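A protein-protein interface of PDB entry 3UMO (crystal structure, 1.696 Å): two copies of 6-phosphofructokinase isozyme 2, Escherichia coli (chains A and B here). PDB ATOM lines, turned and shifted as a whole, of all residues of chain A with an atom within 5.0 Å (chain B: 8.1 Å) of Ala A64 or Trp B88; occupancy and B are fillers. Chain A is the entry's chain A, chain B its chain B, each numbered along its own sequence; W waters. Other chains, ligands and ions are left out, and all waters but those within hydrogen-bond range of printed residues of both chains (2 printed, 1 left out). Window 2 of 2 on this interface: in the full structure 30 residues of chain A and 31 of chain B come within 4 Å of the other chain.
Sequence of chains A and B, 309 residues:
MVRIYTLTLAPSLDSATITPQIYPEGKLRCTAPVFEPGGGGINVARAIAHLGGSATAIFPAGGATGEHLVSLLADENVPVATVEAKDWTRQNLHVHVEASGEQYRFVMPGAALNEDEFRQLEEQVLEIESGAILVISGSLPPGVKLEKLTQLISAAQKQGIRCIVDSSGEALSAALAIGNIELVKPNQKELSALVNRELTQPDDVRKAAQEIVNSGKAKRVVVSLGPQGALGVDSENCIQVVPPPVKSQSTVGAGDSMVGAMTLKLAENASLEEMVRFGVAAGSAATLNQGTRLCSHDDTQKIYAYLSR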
ATOM      1  N   LEU A  13      29.718  16.586  30.274  1.00  0.00           N
ATOM      2  CA  LEU A  13      28.896  15.517  30.820  1.00  0.00           C
ATOM      3  C   LEU A  13      29.655  14.230  30.549  1.00  0.00           C
ATOM      4  O   LEU A  13      29.681  13.743  29.419  1.00  0.00           O
ATOM      5  CB  LEU A  13      27.525  15.461  30.143  1.00  0.00           C
ATOM      6  CG  LEU A  13      26.603  14.355  30.669  1.00  0.00           C
ATOM      7  CD1 LEU A  13      26.170  14.683  32.087  1.00  0.00           C
ATOM      8  CD2 LEU A  13      25.388  14.178  29.764  1.00  0.00           C
ATOM      9  N   PHE A  35      26.406   8.672  33.907  1.00  0.00           N
ATOM     10  CA  PHE A  35      26.809  10.046  33.624  1.00  0.00           C
ATOM     11  C   PHE A  35      27.205  10.784  34.892  1.00  0.00           C
ATOM     12  O   PHE A  35      26.616  10.583  35.953  1.00  0.00           O
ATOM     13  CB  PHE A  35      25.702  10.804  32.888  1.00  0.00           C
ATOM     14  CG  PHE A  35      25.317  10.175  31.581  1.00  0.00           C
ATOM     15  CD1 PHE A  35      26.186  10.204  30.507  1.00  0.00           C
ATOM     16  CD2 PHE A  35      24.093   9.536  31.430  1.00  0.00           C
ATOM     17  CE1 PHE A  35      25.850   9.620  29.295  1.00  0.00           C
ATOM     18  CE2 PHE A  35      23.747   8.943  30.220  1.00  0.00           C
ATOM     19  CZ  PHE A  35      24.630   8.988  29.150  1.00  0.00           C
ATOM     20  N   GLY A  62      24.630  23.486  27.231  1.00  0.00           N
ATOM     21  CA  GLY A  62      23.921  23.450  25.965  1.00  0.00           C
ATOM     22  C   GLY A  62      23.325  22.093  25.655  1.00  0.00           C
ATOM     23  O   GLY A  62      23.936  21.056  25.917  1.00  0.00           O
ATOM     24  N   GLY A  63      22.119  22.103  25.096  1.00  0.00           N
ATOM     25  CA  GLY A  63      21.469  20.878  24.673  1.00  0.00           C
ATOM     26  C   GLY A  63      21.043  19.975  25.812  1.00  0.00           C
ATOM     27  O   GLY A  63      21.093  20.357  26.986  1.00  0.00           O
ATOM     28  N   ALA A  64      20.627  18.764  25.456  1.00  0.00           N
ATOM     29  CA  ALA A  64      20.135  17.795  26.429  1.00  0.00           C
ATOM     30  C   ALA A  64      21.246  17.305  27.349  1.00  0.00           C
ATOM     31  O   ALA A  64      20.994  16.940  28.495  1.00  0.00           O
ATOM     32  CB  ALA A  64      19.480  16.621  25.718  1.00  0.00           C
ATOM     33  N   THR A  65      22.473  17.281  26.841  1.00  0.00           N
ATOM     34  CA  THR A  65      23.609  16.899  27.668  1.00  0.00           C
ATOM     35  C   THR A  65      23.850  17.947  28.742  1.00  0.00           C
ATOM     36  O   THR A  65      24.135  17.614  29.891  1.00  0.00           O
ATOM     37  CB  THR A  65      24.887  16.680  26.834  1.00  0.00           C
ATOM     38  OG1 THR A  65      25.073  17.780  25.934  1.00  0.00           O
ATOM     39  CG2 THR A  65      24.772  15.398  26.029  1.00  0.00           C
ATOM     40  N   GLY A  66      23.727  19.215  28.363  1.00  0.00           N
ATOM     41  CA  GLY A  66      23.836  20.303  29.317  1.00  0.00           C
ATOM     42  C   GLY A  66      22.725  20.259  30.352  1.00  0.00           C
ATOM     43  O   GLY A  66      22.961  20.522  31.538  1.00  0.00           O
ATOM     44  N   GLU A  67      21.515  19.917  29.916  1.00  0.00           N
ATOM     45  CA  GLU A  67      20.388  19.801  30.837  1.00  0.00           C
ATOM     46  C   GLU A  67      20.665  18.717  31.874  1.00  0.00           C
ATOM     47  O   GLU A  67      20.356  18.878  33.057  1.00  0.00           O
ATOM     48  CB  GLU A  67      19.090  19.468  30.090  1.00  0.00           C
ATOM     49  CG  GLU A  67      18.518  20.594  29.250  1.00  0.00           C
ATOM     50  CD  GLU A  67      17.196  20.211  28.603  1.00  0.00           C
ATOM     51  OE1 GLU A  67      17.085  20.322  27.364  1.00  0.00           O
ATOM     52  OE2 GLU A  67      16.271  19.799  29.336  1.00  0.00           O
ATOM     53  N   HIS A  68      21.247  17.612  31.422  1.00  0.00           N
ATOM     54  CA  HIS A  68      21.521  16.495  32.313  1.00  0.00           C
ATOM     55  C   HIS A  68      22.621  16.859  33.296  1.00  0.00           C
ATOM     56  O   HIS A  68      22.562  16.491  34.468  1.00  0.00           O
ATOM     57  CB  HIS A  68      21.897  15.237  31.527  1.00  0.00           C
ATOM     58  CG  HIS A  68      21.770  13.978  32.326  1.00  0.00           C
ATOM     59  ND1 HIS A  68      20.620  13.644  33.003  1.00  0.00           N
ATOM     60  CD2 HIS A  68      22.653  12.979  32.568  1.00  0.00           C
ATOM     61  CE1 HIS A  68      20.793  12.490  33.622  1.00  0.00           C
ATOM     62  NE2 HIS A  68      22.019  12.066  33.376  1.00  0.00           N
ATOM     63  N   GLN A  91      31.166  15.560  25.883  1.00  0.00           N
ATOM     64  CA  GLN A  91      31.298  14.407  26.768  1.00  0.00           C
ATOM     65  C   GLN A  91      32.702  13.819  26.742  1.00  0.00           C
ATOM     66  O   GLN A  91      33.248  13.556  25.664  1.00  0.00           O
ATOM     67  CB  GLN A  91      30.321  13.310  26.348  1.00  0.00           C
ATOM     68  CG  GLN A  91      28.863  13.737  26.240  1.00  0.00           C
ATOM     69  CD  GLN A  91      27.914  12.576  26.494  1.00  0.00           C
ATOM     70  OE1 GLN A  91      27.054  12.266  25.670  1.00  0.00           O
ATOM     71  NE2 GLN A  91      28.073  11.924  27.644  1.00  0.00           N
ATOM     72  N   PRO B  11      20.780   4.150  16.456  1.00  0.00           N
ATOM     73  CA  PRO B  11      21.804   4.897  15.727  1.00  0.00           C
ATOM     74  C   PRO B  11      22.727   5.596  16.710  1.00  0.00           C
ATOM     75  O   PRO B  11      22.480   5.566  17.915  1.00  0.00           O
ATOM     76  CB  PRO B  11      20.986   5.931  14.957  1.00  0.00           C
ATOM     77  CG  PRO B  11      19.803   6.177  15.823  1.00  0.00           C
ATOM     78  CD  PRO B  11      19.511   4.897  16.554  1.00  0.00           C
ATOM     79  N   SER B  12      23.783   6.218  16.206  1.00  0.00           N
ATOM     80  CA  SER B  12      24.654   7.003  17.067  1.00  0.00           C
ATOM     81  C   SER B  12      25.326   8.130  16.296  1.00  0.00           C
ATOM     82  O   SER B  12      25.392   8.102  15.064  1.00  0.00           O
ATOM     83  CB  SER B  12      25.715   6.116  17.730  1.00  0.00           C
ATOM     84  OG  SER B  12      26.582   5.537  16.769  1.00  0.00           O
ATOM     85  N   LEU B  13      25.789   9.135  17.033  1.00  0.00           N
ATOM     86  CA  LEU B  13      26.643  10.174  16.480  1.00  0.00           C
ATOM     87  C   LEU B  13      28.028   9.868  17.022  1.00  0.00           C
ATOM     88  O   LEU B  13      28.331  10.153  18.181  1.00  0.00           O
ATOM     89  CB  LEU B  13      26.203  11.567  16.928  1.00  0.00           C
ATOM     90  CG  LEU B  13      27.106  12.692  16.404  1.00  0.00           C
ATOM     91  CD1 LEU B  13      26.923  12.836  14.897  1.00  0.00           C
ATOM     92  CD2 LEU B  13      26.846  14.013  17.120  1.00  0.00           C
ATOM     93  N   PRO B  60      15.394   6.744  14.730  1.00  0.00           N
ATOM     94  CA  PRO B  60      15.040   7.792  15.692  1.00  0.00           C
ATOM     95  C   PRO B  60      16.209   8.747  15.896  1.00  0.00           C
ATOM     96  O   PRO B  60      17.365   8.321  15.889  1.00  0.00           O
ATOM     97  CB  PRO B  60      14.774   7.010  16.978  1.00  0.00           C
ATOM     98  CG  PRO B  60      15.639   5.788  16.860  1.00  0.00           C
ATOM     99  CD  PRO B  60      15.666   5.452  15.388  1.00  0.00           C
ATOM    100  N   ALA B  61      15.906  10.031  16.054  1.00  0.00           N
ATOM    101  CA  ALA B  61      16.926  11.033  16.325  1.00  0.00           C
ATOM    102  C   ALA B  61      16.465  11.921  17.474  1.00  0.00           C
ATOM    103  O   ALA B  61      15.314  12.348  17.512  1.00  0.00           O
ATOM    104  CB  ALA B  61      17.193  11.870  15.082  1.00  0.00           C
ATOM    105  N   GLY B  62      17.364  12.197  18.414  1.00  0.00           N
ATOM    106  CA  GLY B  62      17.014  13.017  19.561  1.00  0.00           C
ATOM    107  C   GLY B  62      18.076  14.044  19.912  1.00  0.00           C
ATOM    108  O   GLY B  62      19.271  13.765  19.842  1.00  0.00           O
ATOM    109  N   GLY B  63      17.634  15.239  20.292  1.00  0.00           N
ATOM    110  CA  GLY B  63      18.540  16.279  20.748  1.00  0.00           C
ATOM    111  C   GLY B  63      19.457  16.836  19.676  1.00  0.00           C
ATOM    112  O   GLY B  63      19.312  16.533  18.490  1.00  0.00           O
ATOM    113  N   ALA B  64      20.412  17.657  20.102  1.00  0.00           N
ATOM    114  CA  ALA B  64      21.362  18.285  19.187  1.00  0.00           C
ATOM    115  C   ALA B  64      22.251  17.259  18.486  1.00  0.00           C
ATOM    116  O   ALA B  64      22.637  17.447  17.332  1.00  0.00           O
ATOM    117  CB  ALA B  64      22.212  19.312  19.929  1.00  0.00           C
ATOM    118  N   THR B  65      22.585  16.179  19.187  1.00  0.00           N
ATOM    119  CA  THR B  65      23.394  15.126  18.587  1.00  0.00           C
ATOM    120  C   THR B  65      22.627  14.479  17.438  1.00  0.00           C
ATOM    121  O   THR B  65      23.191  14.213  16.376  1.00  0.00           O
ATOM    122  CB  THR B  65      23.835  14.065  19.619  1.00  0.00           C
ATOM    123  OG1 THR B  65      22.712  13.664  20.409  1.00  0.00           O
ATOM    124  CG2 THR B  65      24.910  14.626  20.542  1.00  0.00           C
ATOM    125  N   GLY B  66      21.333  14.254  17.648  1.00  0.00           N
ATOM    126  CA  GLY B  66      20.481  13.691  16.615  1.00  0.00           C
ATOM    127  C   GLY B  66      20.389  14.596  15.402  1.00  0.00           C
ATOM    128  O   GLY B  66      20.412  14.129  14.260  1.00  0.00           O
ATOM    129  N   ALA B  85      12.899  11.575  18.912  1.00  0.00           N
ATOM    130  CA  ALA B  85      12.868  10.814  20.157  1.00  0.00           C
ATOM    131  C   ALA B  85      13.214  11.705  21.343  1.00  0.00           C
ATOM    132  O   ALA B  85      13.973  12.666  21.204  1.00  0.00           O
ATOM    133  CB  ALA B  85      13.830   9.638  20.080  1.00  0.00           C
ATOM    134  N   LYS B  86      12.664  11.376  22.510  1.00  0.00           N
ATOM    135  CA  LYS B  86      12.920  12.142  23.728  1.00  0.00           C
ATOM    136  C   LYS B  86      14.373  12.026  24.188  1.00  0.00           C
ATOM    137  O   LYS B  86      15.011  13.029  24.507  1.00  0.00           O
ATOM    138  CB  LYS B  86      11.995  11.678  24.854  1.00  0.00           C
ATOM    139  CG  LYS B  86      10.521  11.880  24.580  1.00  0.00           C
ATOM    140  CD  LYS B  86      10.048  13.245  25.034  1.00  0.00           C
ATOM    141  CE  LYS B  86       8.695  13.561  24.428  1.00  0.00           C
ATOM    142  NZ  LYS B  86       8.785  13.543  22.942  1.00  0.00           N
ATOM    143  N   ASP B  87      14.880  10.797  24.238  1.00  0.00           N
ATOM    144  CA  ASP B  87      16.238  10.538  24.709  1.00  0.00           C
ATOM    145  C   ASP B  87      17.255  10.886  23.622  1.00  0.00           C
ATOM    146  O   ASP B  87      17.079  10.518  22.457  1.00  0.00           O
ATOM    147  CB  ASP B  87      16.377   9.076  25.131  1.00  0.00           C
ATOM    148  CG  ASP B  87      17.592   8.834  25.997  1.00  0.00           C
ATOM    149  OD1 ASP B  87      18.171   9.822  26.497  1.00  0.00           O
ATOM    150  OD2 ASP B  87      17.960   7.654  26.184  1.00  0.00           O
ATOM    151  N   TRP B  88      18.318  11.594  23.998  1.00  0.00           N
ATOM    152  CA  TRP B  88      19.245  12.140  23.005  1.00  0.00           C
ATOM    153  C   TRP B  88      20.085  11.067  22.316  1.00  0.00           C
ATOM    154  O   TRP B  88      20.473  10.076  22.936  1.00  0.00           O
ATOM    155  CB  TRP B  88      20.138  13.237  23.615  1.00  0.00           C
ATOM    156  CG  TRP B  88      21.302  12.746  24.466  1.00  0.00           C
ATOM    157  CD1 TRP B  88      22.519  12.290  24.022  1.00  0.00           C
ATOM    158  CD2 TRP B  88      21.360  12.701  25.902  1.00  0.00           C
ATOM    159  NE1 TRP B  88      23.317  11.952  25.093  1.00  0.00           N
ATOM    160  CE2 TRP B  88      22.635  12.194  26.248  1.00  0.00           C
ATOM    161  CE3 TRP B  88      20.458  13.031  26.913  1.00  0.00           C
ATOM    162  CZ2 TRP B  88      23.018  12.014  27.580  1.00  0.00           C
ATOM    163  CZ3 TRP B  88      20.847  12.851  28.231  1.00  0.00           C
ATOM    164  CH2 TRP B  88      22.115  12.346  28.553  1.00  0.00           C
ATOM    165  N   THR B  89      20.356  11.273  21.030  1.00  0.00           N
ATOM    166  CA  THR B  89      21.157  10.327  20.251  1.00  0.00           C
ATOM    167  C   THR B  89      22.527  10.118  20.888  1.00  0.00           C
ATOM    168  O   THR B  89      23.271  11.072  21.127  1.00  0.00           O
ATOM    169  CB  THR B  89      21.312  10.796  18.792  1.00  0.00           C
ATOM    170  OG1 THR B  89      20.020  10.838  18.176  1.00  0.00           O
ATOM    171  CG2 THR B  89      22.208   9.844  18.006  1.00  0.00           C
ATOM    172  N   ARG B  90      22.849   8.862  21.176  1.00  0.00           N
ATOM    173  CA  ARG B  90      24.055   8.543  21.927  1.00  0.00           C
ATOM    174  C   ARG B  90      25.303   8.560  21.047  1.00  0.00           C
ATOM    175  O   ARG B  90      25.213   8.614  19.820  1.00  0.00           O
ATOM    176  CB  ARG B  90      23.908   7.190  22.627  1.00  0.00           C
ATOM    177  CG  ARG B  90      22.863   7.192  23.740  1.00  0.00           C
ATOM    178  CD  ARG B  90      23.279   8.099  24.887  1.00  0.00           C
ATOM    179  NE  ARG B  90      22.507   7.842  26.102  1.00  0.00           N
ATOM    180  CZ  ARG B  90      21.404   8.496  26.448  1.00  0.00           C
ATOM    181  NH1 ARG B  90      20.778   8.181  27.578  1.00  0.00           N
ATOM    182  NH2 ARG B  90      20.924   9.463  25.669  1.00  0.00           N
ATOM    183  N   GLN B  91      26.462   8.519  21.691  1.00  0.00           N
ATOM    184  CA  GLN B  91      27.733   8.635  20.996  1.00  0.00           C
ATOM    185  C   GLN B  91      28.667   7.495  21.370  1.00  0.00           C
ATOM    186  O   GLN B  91      28.863   7.200  22.553  1.00  0.00           O
ATOM    187  CB  GLN B  91      28.397   9.964  21.358  1.00  0.00           C
ATOM    188  CG  GLN B  91      27.478  11.167  21.226  1.00  0.00           C
ATOM    189  CD  GLN B  91      28.114  12.444  21.741  1.00  0.00           C
ATOM    190  OE1 GLN B  91      27.856  12.869  22.871  1.00  0.00           O
ATOM    191  NE2 GLN B  91      28.949  13.063  20.912  1.00  0.00           N
ATOM    192  N   PRO B 109      25.471   1.325  24.308  1.00  0.00           N
ATOM    193  CA  PRO B 109      24.121   1.176  23.755  1.00  0.00           C
ATOM    194  C   PRO B 109      23.574   2.466  23.140  1.00  0.00           C
ATOM    195  O   PRO B 109      24.064   3.575  23.411  1.00  0.00           O
ATOM    196  CB  PRO B 109      23.283   0.796  24.981  1.00  0.00           C
ATOM    197  CG  PRO B 109      24.248   0.162  25.913  1.00  0.00           C
ATOM    198  CD  PRO B 109      25.525   0.932  25.728  1.00  0.00           C
ATOM    199  N   GLY B 110      22.558   2.311  22.300  1.00  0.00           N
ATOM    200  CA  GLY B 110      21.879   3.458  21.733  1.00  0.00           C
ATOM    201  C   GLY B 110      20.916   4.060  22.738  1.00  0.00           C
ATOM    202  O   GLY B 110      20.717   3.520  23.829  1.00  0.00           O
ATOM    203  N   ALA B 111      20.317   5.188  22.371  1.00  0.00           N
ATOM    204  CA  ALA B 111      19.364   5.863  23.241  1.00  0.00           C
ATOM    205  C   ALA B 111      18.101   5.028  23.419  1.00  0.00           C
ATOM    206  O   ALA B 111      17.783   4.180  22.587  1.00  0.00           O
ATOM    207  CB  ALA B 111      19.014   7.232  22.689  1.00  0.00           C
ATOM    208  N   ALA B 112      17.379   5.274  24.504  1.00  0.00           N
ATOM    209  CA  ALA B 112      16.127   4.562  24.749  1.00  0.00           C
ATOM    210  C   ALA B 112      15.045   4.980  23.754  1.00  0.00           C
ATOM    211  O   ALA B 112      15.070   6.091  23.218  1.00  0.00           O
ATOM    212  CB  ALA B 112      15.648   4.783  26.177  1.00  0.00           C
HETATM  213  O   HOH W   1      19.715  18.778  22.691  1.00  0.00           O
HETATM  214  O   HOH W   2      30.872  14.996  22.719  1.00  0.00           O
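OE1 of Gln B91 lies close to OE1 of Gln A91 (3.0 Å).
The backbone carbonyl oxygen (O) of Leu A13 is in hydrogen-bond range of the side-chain amide nitrogen (NE2) of Gln A91 (3.0 Å). The side-chain hydroxyl (OG1) of Thr A65 is in hydrogen-bond range of the backbone carbonyl oxygen (O) of Gly A62, 3.5 Å away. The backbone NH (N) of Leu B13 sits at hydrogen-bond distance from the backbone carbonyl oxygen (O) of Arg B90 (2.9 Å). The side-chain carboxylate (OD1) of Asp B87 is in salt-bridge range of the guanidinium group (NH2) of Arg B90, at 2.9 Å. The guanidinium group (NH2) of Arg B90 sits at hydrogen-bond distance from the backbone carbonyl oxygen (O) of Trp B88 (2.8 Å).
Trp B88 touches Leu A13 (CZ2 to CD2, 3.9 Å). CZ of Phe A35 touches CZ2 of Trp B88 (3.8 Å). Phe A35 touches Arg B90 (CZ to NE, 3.9 Å). Ala A64 touches Trp B88 (CB to CE3, 3.9 Å). Thr A65 touches Trp B88 (CG2 to NE1, 3.9 Å). Trp B88 touches Gln A91 (NE1 to OE1, 3.8 Å).
Ala A64 touches just one residue of chain B: Trp B88. Trp B88 touches just these residues of chain A: Leu A13, Phe A35, Ala A64, Thr A65 and Gln A91. Of the printed residues of chain A, Arg B90 touches Phe A35 (3.9 Å). Of the printed residues of chain B, Leu A13 touches Trp B88. Printed residues of chain B within 4 Å of Phe A35: Trp B88 and Arg B90. Of the printed residues of chain B, Thr A65 touches Trp B88 (3.9 Å). The nearest residue of chain B that does not touch Ala A64 is Gly B63 (5.1 Å).
Printed residues of chain B that touch a printed residue of chain A: Trp B88, Arg B90 and Gln B91. Along chain B the printed residues that touch a printed residue of chain A span positions 88 to 91. Of the 10 printed residues of chain A, 5 touch a printed residue of chain B. Hydrophobic or aromatic side chains of chain A that line the printed part of chain B: Leu A13, Phe A35 and Ala A64. Among the printed residues, 7 pairs touch across the chains. Among the printed residues, no Asp or Glu carboxylate lies within 4 Å of a Lys or Arg side-chain nitrogen of the other chain.
Gln B91 touches its own counterpart, Gln A91.
Water W1 bridges the backbone NH (N) of Ala B64 (2.9 Å) and the backbone NH (N) of Ala A64 (2.9 Å). Water W2 bridges the backbone NH of Gln A91 (3.2 Å) and the side-chain amide nitrogen of Gln B91 (3.3 Å).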
